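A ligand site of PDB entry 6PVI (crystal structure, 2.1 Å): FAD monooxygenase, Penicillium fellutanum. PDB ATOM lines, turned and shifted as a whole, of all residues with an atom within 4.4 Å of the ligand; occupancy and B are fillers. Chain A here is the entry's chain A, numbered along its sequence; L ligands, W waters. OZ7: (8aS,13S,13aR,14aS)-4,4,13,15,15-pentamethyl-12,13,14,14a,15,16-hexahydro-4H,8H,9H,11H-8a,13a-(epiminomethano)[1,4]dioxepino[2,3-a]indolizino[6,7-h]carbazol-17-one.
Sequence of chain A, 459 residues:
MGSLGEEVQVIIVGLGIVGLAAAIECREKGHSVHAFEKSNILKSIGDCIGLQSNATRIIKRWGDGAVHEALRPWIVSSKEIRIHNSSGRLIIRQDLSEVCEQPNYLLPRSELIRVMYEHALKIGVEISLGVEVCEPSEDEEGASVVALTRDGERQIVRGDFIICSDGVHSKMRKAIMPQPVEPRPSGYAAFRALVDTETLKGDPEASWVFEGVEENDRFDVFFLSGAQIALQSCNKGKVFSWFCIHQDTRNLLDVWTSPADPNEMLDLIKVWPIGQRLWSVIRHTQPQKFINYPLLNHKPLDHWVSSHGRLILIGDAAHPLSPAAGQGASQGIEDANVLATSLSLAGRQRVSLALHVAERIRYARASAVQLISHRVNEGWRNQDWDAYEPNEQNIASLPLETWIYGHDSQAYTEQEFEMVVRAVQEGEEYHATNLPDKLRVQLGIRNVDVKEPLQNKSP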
ATOM      1  N   LEU A  51     -12.269 -24.201 -20.034  1.00  0.00           N
ATOM      2  CA  LEU A  51     -11.522 -23.232 -19.242  1.00  0.00           C
ATOM      3  C   LEU A  51     -10.558 -22.489 -20.168  1.00  0.00           C
ATOM      4  O   LEU A  51      -9.646 -23.091 -20.740  1.00  0.00           O
ATOM      5  CB  LEU A  51     -10.750 -23.898 -18.110  1.00  0.00           C
ATOM      6  CG  LEU A  51     -11.527 -24.409 -16.876  1.00  0.00           C
ATOM      7  CD1 LEU A  51     -10.571 -25.076 -15.919  1.00  0.00           C
ATOM      8  CD2 LEU A  51     -12.321 -23.304 -16.199  1.00  0.00           C
ATOM      9  N   GLN A  52     -10.766 -21.185 -20.301  1.00  0.00           N
ATOM     10  CA  GLN A  52      -9.920 -20.379 -21.153  1.00  0.00           C
ATOM     11  C   GLN A  52      -8.695 -19.808 -20.398  1.00  0.00           C
ATOM     12  O   GLN A  52      -8.553 -19.940 -19.185  1.00  0.00           O
ATOM     13  CB  GLN A  52     -10.754 -19.272 -21.765  1.00  0.00           C
ATOM     14  CG  GLN A  52     -11.681 -19.823 -22.814  1.00  0.00           C
ATOM     15  CD  GLN A  52     -12.413 -18.742 -23.532  1.00  0.00           C
ATOM     16  OE1 GLN A  52     -13.561 -18.464 -23.213  1.00  0.00           O
ATOM     17  NE2 GLN A  52     -11.761 -18.103 -24.496  1.00  0.00           N
ATOM     18  N   VAL A  76      -6.562 -28.044 -24.887  1.00  0.00           N
ATOM     19  CA  VAL A  76      -7.225 -27.924 -26.174  1.00  0.00           C
ATOM     20  C   VAL A  76      -6.199 -27.826 -27.279  1.00  0.00           C
ATOM     21  O   VAL A  76      -5.271 -27.005 -27.210  1.00  0.00           O
ATOM     22  CB  VAL A  76      -8.177 -26.722 -26.197  1.00  0.00           C
ATOM     23  CG1 VAL A  76      -8.646 -26.448 -27.625  1.00  0.00           C
ATOM     24  CG2 VAL A  76      -9.384 -26.975 -25.288  1.00  0.00           C
ATOM     25  N   VAL A  99      -6.250 -17.432 -29.402  1.00  0.00           N
ATOM     26  CA  VAL A  99      -7.037 -17.896 -28.266  1.00  0.00           C
ATOM     27  C   VAL A  99      -6.287 -19.005 -27.541  1.00  0.00           C
ATOM     28  O   VAL A  99      -6.322 -19.090 -26.302  1.00  0.00           O
ATOM     29  CB  VAL A  99      -8.434 -18.342 -28.727  1.00  0.00           C
ATOM     30  CG1 VAL A  99      -9.043 -19.332 -27.756  1.00  0.00           C
ATOM     31  CG2 VAL A  99      -9.332 -17.140 -28.903  1.00  0.00           C
ATOM     32  N   CYS A 100      -5.558 -19.848 -28.281  1.00  0.00           N
ATOM     33  CA  CYS A 100      -4.869 -21.002 -27.720  1.00  0.00           C
ATOM     34  C   CYS A 100      -3.366 -20.810 -27.656  1.00  0.00           C
ATOM     35  O   CYS A 100      -2.638 -21.800 -27.531  1.00  0.00           O
ATOM     36  CB  CYS A 100      -5.196 -22.269 -28.510  1.00  0.00           C
ATOM     37  SG  CYS A 100      -6.957 -22.728 -28.522  1.00  0.00           S
ATOM     38  N   ASN A 104      -5.626 -23.691 -23.015  1.00  0.00           N
ATOM     39  CA  ASN A 104      -7.039 -23.792 -22.670  1.00  0.00           C
ATOM     40  C   ASN A 104      -7.355 -25.234 -22.326  1.00  0.00           C
ATOM     41  O   ASN A 104      -6.733 -26.163 -22.864  1.00  0.00           O
ATOM     42  CB  ASN A 104      -7.941 -23.343 -23.836  1.00  0.00           C
ATOM     43  CG  ASN A 104      -7.719 -21.891 -24.236  1.00  0.00           C
ATOM     44  OD1 ASN A 104      -8.547 -21.043 -23.969  1.00  0.00           O
ATOM     45  ND2 ASN A 104      -6.597 -21.620 -24.889  1.00  0.00           N
ATOM     46  N   TYR A 105      -8.313 -25.445 -21.436  1.00  0.00           N
ATOM     47  CA  TYR A 105      -8.757 -26.792 -21.113  1.00  0.00           C
ATOM     48  C   TYR A 105     -10.178 -27.016 -21.580  1.00  0.00           C
ATOM     49  O   TYR A 105     -10.991 -26.094 -21.646  1.00  0.00           O
ATOM     50  CB  TYR A 105      -8.723 -27.085 -19.605  1.00  0.00           C
ATOM     51  CG  TYR A 105      -7.390 -26.905 -18.912  1.00  0.00           C
ATOM     52  CD1 TYR A 105      -6.220 -27.488 -19.398  1.00  0.00           C
ATOM     53  CD2 TYR A 105      -7.307 -26.147 -17.749  1.00  0.00           C
ATOM     54  CE1 TYR A 105      -5.019 -27.314 -18.725  1.00  0.00           C
ATOM     55  CE2 TYR A 105      -6.134 -25.962 -17.089  1.00  0.00           C
ATOM     56  CZ  TYR A 105      -4.993 -26.537 -17.574  1.00  0.00           C
ATOM     57  OH  TYR A 105      -3.830 -26.323 -16.875  1.00  0.00           O
ATOM     58  N   LEU A 106     -10.482 -28.273 -21.899  1.00  0.00           N
ATOM     59  CA  LEU A 106     -11.860 -28.697 -22.133  1.00  0.00           C
ATOM     60  C   LEU A 106     -11.914 -30.136 -21.670  1.00  0.00           C
ATOM     61  O   LEU A 106     -11.180 -30.982 -22.192  1.00  0.00           O
ATOM     62  CB  LEU A 106     -12.263 -28.603 -23.605  1.00  0.00           C
ATOM     63  CG  LEU A 106     -13.658 -29.202 -23.849  1.00  0.00           C
ATOM     64  CD1 LEU A 106     -14.785 -28.232 -23.449  1.00  0.00           C
ATOM     65  CD2 LEU A 106     -13.807 -29.638 -25.287  1.00  0.00           C
ATOM     66  N   PHE A 219     -13.800 -29.364 -33.396  1.00  0.00           N
ATOM     67  CA  PHE A 219     -14.641 -28.262 -32.919  1.00  0.00           C
ATOM     68  C   PHE A 219     -15.503 -27.772 -34.098  1.00  0.00           C
ATOM     69  O   PHE A 219     -15.124 -26.844 -34.815  1.00  0.00           O
ATOM     70  CB  PHE A 219     -13.830 -27.133 -32.313  1.00  0.00           C
ATOM     71  CG  PHE A 219     -14.665 -26.188 -31.523  1.00  0.00           C
ATOM     72  CD1 PHE A 219     -14.797 -26.309 -30.162  1.00  0.00           C
ATOM     73  CD2 PHE A 219     -15.374 -25.197 -32.151  1.00  0.00           C
ATOM     74  CE1 PHE A 219     -15.600 -25.429 -29.452  1.00  0.00           C
ATOM     75  CE2 PHE A 219     -16.171 -24.324 -31.436  1.00  0.00           C
ATOM     76  CZ  PHE A 219     -16.272 -24.447 -30.088  1.00  0.00           C
ATOM     77  N   VAL A 221     -19.354 -26.442 -35.433  1.00  0.00           N
ATOM     78  CA  VAL A 221     -20.591 -25.776 -35.074  1.00  0.00           C
ATOM     79  C   VAL A 221     -21.534 -25.845 -36.276  1.00  0.00           C
ATOM     80  O   VAL A 221     -21.083 -25.797 -37.428  1.00  0.00           O
ATOM     81  CB  VAL A 221     -20.322 -24.315 -34.662  1.00  0.00           C
ATOM     82  CG1 VAL A 221     -21.616 -23.564 -34.540  1.00  0.00           C
ATOM     83  CG2 VAL A 221     -19.497 -24.285 -33.355  1.00  0.00           C
ATOM     84  N   GLN A 228     -28.839 -24.235 -32.925  1.00  0.00           N
ATOM     85  CA  GLN A 228     -27.404 -24.005 -32.967  1.00  0.00           C
ATOM     86  C   GLN A 228     -26.755 -25.216 -32.324  1.00  0.00           C
ATOM     87  O   GLN A 228     -27.080 -25.570 -31.195  1.00  0.00           O
ATOM     88  CB  GLN A 228     -27.043 -22.713 -32.232  1.00  0.00           C
ATOM     89  CG  GLN A 228     -27.624 -21.431 -32.883  1.00  0.00           C
ATOM     90  CD  GLN A 228     -29.128 -21.222 -32.645  1.00  0.00           C
ATOM     91  OE1 GLN A 228     -29.615 -21.362 -31.521  1.00  0.00           O
ATOM     92  NE2 GLN A 228     -29.863 -20.866 -33.704  1.00  0.00           N
ATOM     93  N   ILE A 229     -25.890 -25.894 -33.070  1.00  0.00           N
ATOM     94  CA  ILE A 229     -25.287 -27.149 -32.619  1.00  0.00           C
ATOM     95  C   ILE A 229     -23.778 -27.011 -32.620  1.00  0.00           C
ATOM     96  O   ILE A 229     -23.196 -26.520 -33.604  1.00  0.00           O
ATOM     97  CB  ILE A 229     -25.696 -28.333 -33.507  1.00  0.00           C
ATOM     98  CG1 ILE A 229     -27.207 -28.555 -33.453  1.00  0.00           C
ATOM     99  CG2 ILE A 229     -24.946 -29.562 -33.081  1.00  0.00           C
ATOM    100  CD1 ILE A 229     -27.682 -29.687 -34.328  1.00  0.00           C
ATOM    101  N   ALA A 230     -23.139 -27.473 -31.546  1.00  0.00           N
ATOM    102  CA  ALA A 230     -21.691 -27.621 -31.495  1.00  0.00           C
ATOM    103  C   ALA A 230     -21.334 -29.070 -31.222  1.00  0.00           C
ATOM    104  O   ALA A 230     -22.119 -29.824 -30.632  1.00  0.00           O
ATOM    105  CB  ALA A 230     -21.076 -26.711 -30.433  1.00  0.00           C
ATOM    106  N   GLN A 232     -17.705 -31.394 -30.113  1.00  0.00           N
ATOM    107  CA  GLN A 232     -16.347 -31.233 -29.636  1.00  0.00           C
ATOM    108  C   GLN A 232     -15.762 -32.575 -29.225  1.00  0.00           C
ATOM    109  O   GLN A 232     -16.457 -33.414 -28.636  1.00  0.00           O
ATOM    110  CB  GLN A 232     -16.295 -30.303 -28.437  1.00  0.00           C
ATOM    111  CG  GLN A 232     -16.655 -28.895 -28.732  1.00  0.00           C
ATOM    112  CD  GLN A 232     -16.557 -28.050 -27.492  1.00  0.00           C
ATOM    113  OE1 GLN A 232     -15.624 -27.283 -27.329  1.00  0.00           O
ATOM    114  NE2 GLN A 232     -17.513 -28.220 -26.580  1.00  0.00           N
ATOM    115  N   PHE A 243     -23.832 -30.068 -27.961  1.00  0.00           N
ATOM    116  CA  PHE A 243     -24.644 -29.007 -27.399  1.00  0.00           C
ATOM    117  C   PHE A 243     -25.585 -28.592 -28.512  1.00  0.00           C
ATOM    118  O   PHE A 243     -25.128 -28.390 -29.647  1.00  0.00           O
ATOM    119  CB  PHE A 243     -23.726 -27.853 -26.971  1.00  0.00           C
ATOM    120  CG  PHE A 243     -24.303 -26.939 -25.939  1.00  0.00           C
ATOM    121  CD1 PHE A 243     -23.641 -26.748 -24.722  1.00  0.00           C
ATOM    122  CD2 PHE A 243     -25.466 -26.233 -26.176  1.00  0.00           C
ATOM    123  CE1 PHE A 243     -24.146 -25.877 -23.767  1.00  0.00           C
ATOM    124  CE2 PHE A 243     -25.959 -25.355 -25.226  1.00  0.00           C
ATOM    125  CZ  PHE A 243     -25.307 -25.189 -24.026  1.00  0.00           C
ATOM    126  N   ILE A 245     -28.716 -25.745 -29.044  1.00  0.00           N
ATOM    127  CA  ILE A 245     -29.636 -24.702 -28.571  1.00  0.00           C
ATOM    128  C   ILE A 245     -30.844 -24.651 -29.503  1.00  0.00           C
ATOM    129  O   ILE A 245     -30.705 -24.619 -30.722  1.00  0.00           O
ATOM    130  CB  ILE A 245     -28.961 -23.334 -28.485  1.00  0.00           C
ATOM    131  CG1 ILE A 245     -28.073 -23.285 -27.233  1.00  0.00           C
ATOM    132  CG2 ILE A 245     -29.989 -22.213 -28.399  1.00  0.00           C
ATOM    133  CD1 ILE A 245     -27.236 -22.046 -27.158  1.00  0.00           C
ATOM    134  N   ALA A 324     -23.523 -21.889 -22.327  1.00  0.00           N
ATOM    135  CA  ALA A 324     -23.051 -21.574 -23.668  1.00  0.00           C
ATOM    136  C   ALA A 324     -22.344 -20.213 -23.740  1.00  0.00           C
ATOM    137  O   ALA A 324     -22.130 -19.696 -24.834  1.00  0.00           O
ATOM    138  CB  ALA A 324     -24.231 -21.593 -24.631  1.00  0.00           C
ATOM    139  N   ALA A 325     -21.976 -19.623 -22.607  1.00  0.00           N
ATOM    140  CA  ALA A 325     -21.138 -18.432 -22.670  1.00  0.00           C
ATOM    141  C   ALA A 325     -19.779 -18.748 -23.279  1.00  0.00           C
ATOM    142  O   ALA A 325     -19.318 -18.060 -24.203  1.00  0.00           O
ATOM    143  CB  ALA A 325     -20.973 -17.824 -21.275  1.00  0.00           C
ATOM    144  N   GLY A 326     -19.138 -19.802 -22.791  1.00  0.00           N
ATOM    145  CA  GLY A 326     -17.715 -20.007 -22.966  1.00  0.00           C
ATOM    146  C   GLY A 326     -16.883 -19.468 -21.823  1.00  0.00           C
ATOM    147  O   GLY A 326     -15.765 -19.961 -21.596  1.00  0.00           O
ATOM    148  N   ASN A 377     -25.778 -14.663 -27.496  1.00  0.00           N
ATOM    149  CA  ASN A 377     -26.713 -15.798 -27.473  1.00  0.00           C
ATOM    150  C   ASN A 377     -28.094 -15.396 -27.978  1.00  0.00           C
ATOM    151  O   ASN A 377     -28.810 -16.212 -28.571  1.00  0.00           O
ATOM    152  CB  ASN A 377     -26.806 -16.407 -26.072  1.00  0.00           C
ATOM    153  CG  ASN A 377     -25.853 -17.582 -25.867  1.00  0.00           C
ATOM    154  OD1 ASN A 377     -26.098 -18.698 -26.319  1.00  0.00           O
ATOM    155  ND2 ASN A 377     -24.756 -17.329 -25.151  1.00  0.00           N
ATOM    156  N   ILE A 395     -25.951 -17.605 -32.600  1.00  0.00           N
ATOM    157  CA  ILE A 395     -24.929 -17.790 -31.564  1.00  0.00           C
ATOM    158  C   ILE A 395     -23.777 -18.638 -32.085  1.00  0.00           C
ATOM    159  O   ILE A 395     -23.936 -19.861 -32.231  1.00  0.00           O
ATOM    160  CB  ILE A 395     -25.484 -18.465 -30.297  1.00  0.00           C
ATOM    161  CG1 ILE A 395     -26.900 -17.990 -29.951  1.00  0.00           C
ATOM    162  CG2 ILE A 395     -24.535 -18.244 -29.130  1.00  0.00           C
ATOM    163  CD1 ILE A 395     -28.013 -18.880 -30.420  1.00  0.00           C
ATOM    164  N   SER A 397     -20.223 -18.596 -30.902  1.00  0.00           N
ATOM    165  CA  SER A 397     -18.990 -18.667 -30.118  1.00  0.00           C
ATOM    166  C   SER A 397     -17.830 -18.003 -30.862  1.00  0.00           C
ATOM    167  O   SER A 397     -16.767 -18.582 -31.054  1.00  0.00           O
ATOM    168  CB  SER A 397     -18.623 -20.107 -29.759  1.00  0.00           C
ATOM    169  OG  SER A 397     -17.325 -20.169 -29.200  1.00  0.00           O
HETATM  170  C1  OZ7 L   1     -22.559 -23.691 -28.399  1.00  0.00           C
HETATM  171  C2  OZ7 L   1     -23.630 -24.302 -29.375  1.00  0.00           C
HETATM  172  O1  OZ7 L   1     -14.373 -24.721 -25.466  1.00  0.00           O
HETATM  173  N   OZ7 L   1     -21.811 -21.762 -27.243  1.00  0.00           N
HETATM  174  C   OZ7 L   1     -22.897 -22.321 -27.788  1.00  0.00           C
HETATM  175  O   OZ7 L   1     -24.000 -21.787 -27.796  1.00  0.00           O
HETATM  176  C10 OZ7 L   1     -19.446 -21.722 -26.581  1.00  0.00           C
HETATM  177  C11 OZ7 L   1     -18.260 -22.609 -26.346  1.00  0.00           C
HETATM  178  C12 OZ7 L   1     -18.349 -23.953 -26.183  1.00  0.00           C
HETATM  179  C13 OZ7 L   1     -19.610 -24.786 -26.297  1.00  0.00           C
HETATM  180  C14 OZ7 L   1     -19.789 -25.565 -24.992  1.00  0.00           C
HETATM  181  C15 OZ7 L   1     -19.364 -25.807 -27.423  1.00  0.00           C
HETATM  182  C16 OZ7 L   1     -16.178 -23.445 -25.971  1.00  0.00           C
HETATM  183  C17 OZ7 L   1     -16.870 -22.257 -26.235  1.00  0.00           C
HETATM  184  C18 OZ7 L   1     -16.141 -21.075 -26.376  1.00  0.00           C
HETATM  185  C19 OZ7 L   1     -14.769 -21.086 -26.282  1.00  0.00           C
HETATM  186  C20 OZ7 L   1     -14.075 -22.265 -26.046  1.00  0.00           C
HETATM  187  C21 OZ7 L   1     -14.797 -23.451 -25.845  1.00  0.00           C
HETATM  188  C22 OZ7 L   1     -13.236 -25.251 -26.056  1.00  0.00           C
HETATM  189  C23 OZ7 L   1     -12.091 -24.624 -26.151  1.00  0.00           C
HETATM  190  C24 OZ7 L   1     -11.797 -23.247 -25.610  1.00  0.00           C
HETATM  191  C25 OZ7 L   1     -10.494 -22.735 -26.216  1.00  0.00           C
HETATM  192  C26 OZ7 L   1     -11.723 -23.273 -24.102  1.00  0.00           C
HETATM  193  C3  OZ7 L   1     -25.056 -24.409 -28.868  1.00  0.00           C
HETATM  194  C4  OZ7 L   1     -23.496 -23.453 -30.651  1.00  0.00           C
HETATM  195  C5  OZ7 L   1     -22.086 -22.885 -30.574  1.00  0.00           C
HETATM  196  C6  OZ7 L   1     -20.333 -22.775 -28.813  1.00  0.00           C
HETATM  197  C7  OZ7 L   1     -20.544 -22.498 -27.324  1.00  0.00           C
HETATM  198  C8  OZ7 L   1     -20.832 -23.866 -26.583  1.00  0.00           C
HETATM  199  C9  OZ7 L   1     -22.005 -24.598 -27.279  1.00  0.00           C
HETATM  200  N1  OZ7 L   1     -21.483 -23.488 -29.373  1.00  0.00           N
HETATM  201  N2  OZ7 L   1     -17.098 -24.478 -25.942  1.00  0.00           N
HETATM  202  O2  OZ7 L   1     -12.692 -22.237 -26.163  1.00  0.00           O
HETATM  203  O   HOH W   1     -19.897 -18.427 -26.785  1.00  0.00           O
HETATM  204  O   HOH W   2     -19.515 -22.971 -22.832  1.00  0.00           O
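OE1 of Gln 232 lies close to O1 of the ligand (3.4 Å).
N of the ligand sits at hydrogen-bond distance from O of Ala 324, at 3.2 Å.
O of Gln 228 lies within hydrogen-bond range of N of Ile 245 (2.7 Å).
The backbone NH (N) of Ala 230 lies within hydrogen-bond range of the backbone carbonyl oxygen (O) of Phe 243.
N of Tyr 105 lies within hydrogen-bond range of O of Leu 51 (2.8 Å).
The backbone carbonyl oxygen of Asn 104 is in hydrogen-bond range of the backbone NH of Val 76, 2.8 Å away.
The side-chain amide oxygen of Gln 52 lies close to the backbone carbonyl oxygen of Gly 326 (3.1 Å).
O of Val 99 sits at hydrogen-bond distance from ND2 of Asn 104 (2.9 Å).
Residues that only touch the ligand: Ser 397 (3.2 Å), Phe 243 (3.3 Å), Gln 228 (3.3 Å), Ile 245 (3.3 Å), Ala 230 (3.4 Å), Asn 104 (3.4 Å), Gln 52 (3.7 Å), Val 76 (3.7 Å), Tyr 105 (3.8 Å), Ile 395 (3.8 Å), Gly 326 (3.9 Å), Phe 219 (3.9 Å) and Leu 51 (3.96 Å).
The nearest printed residue that does not touch the ligand is Val 99 (4.01 Å).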
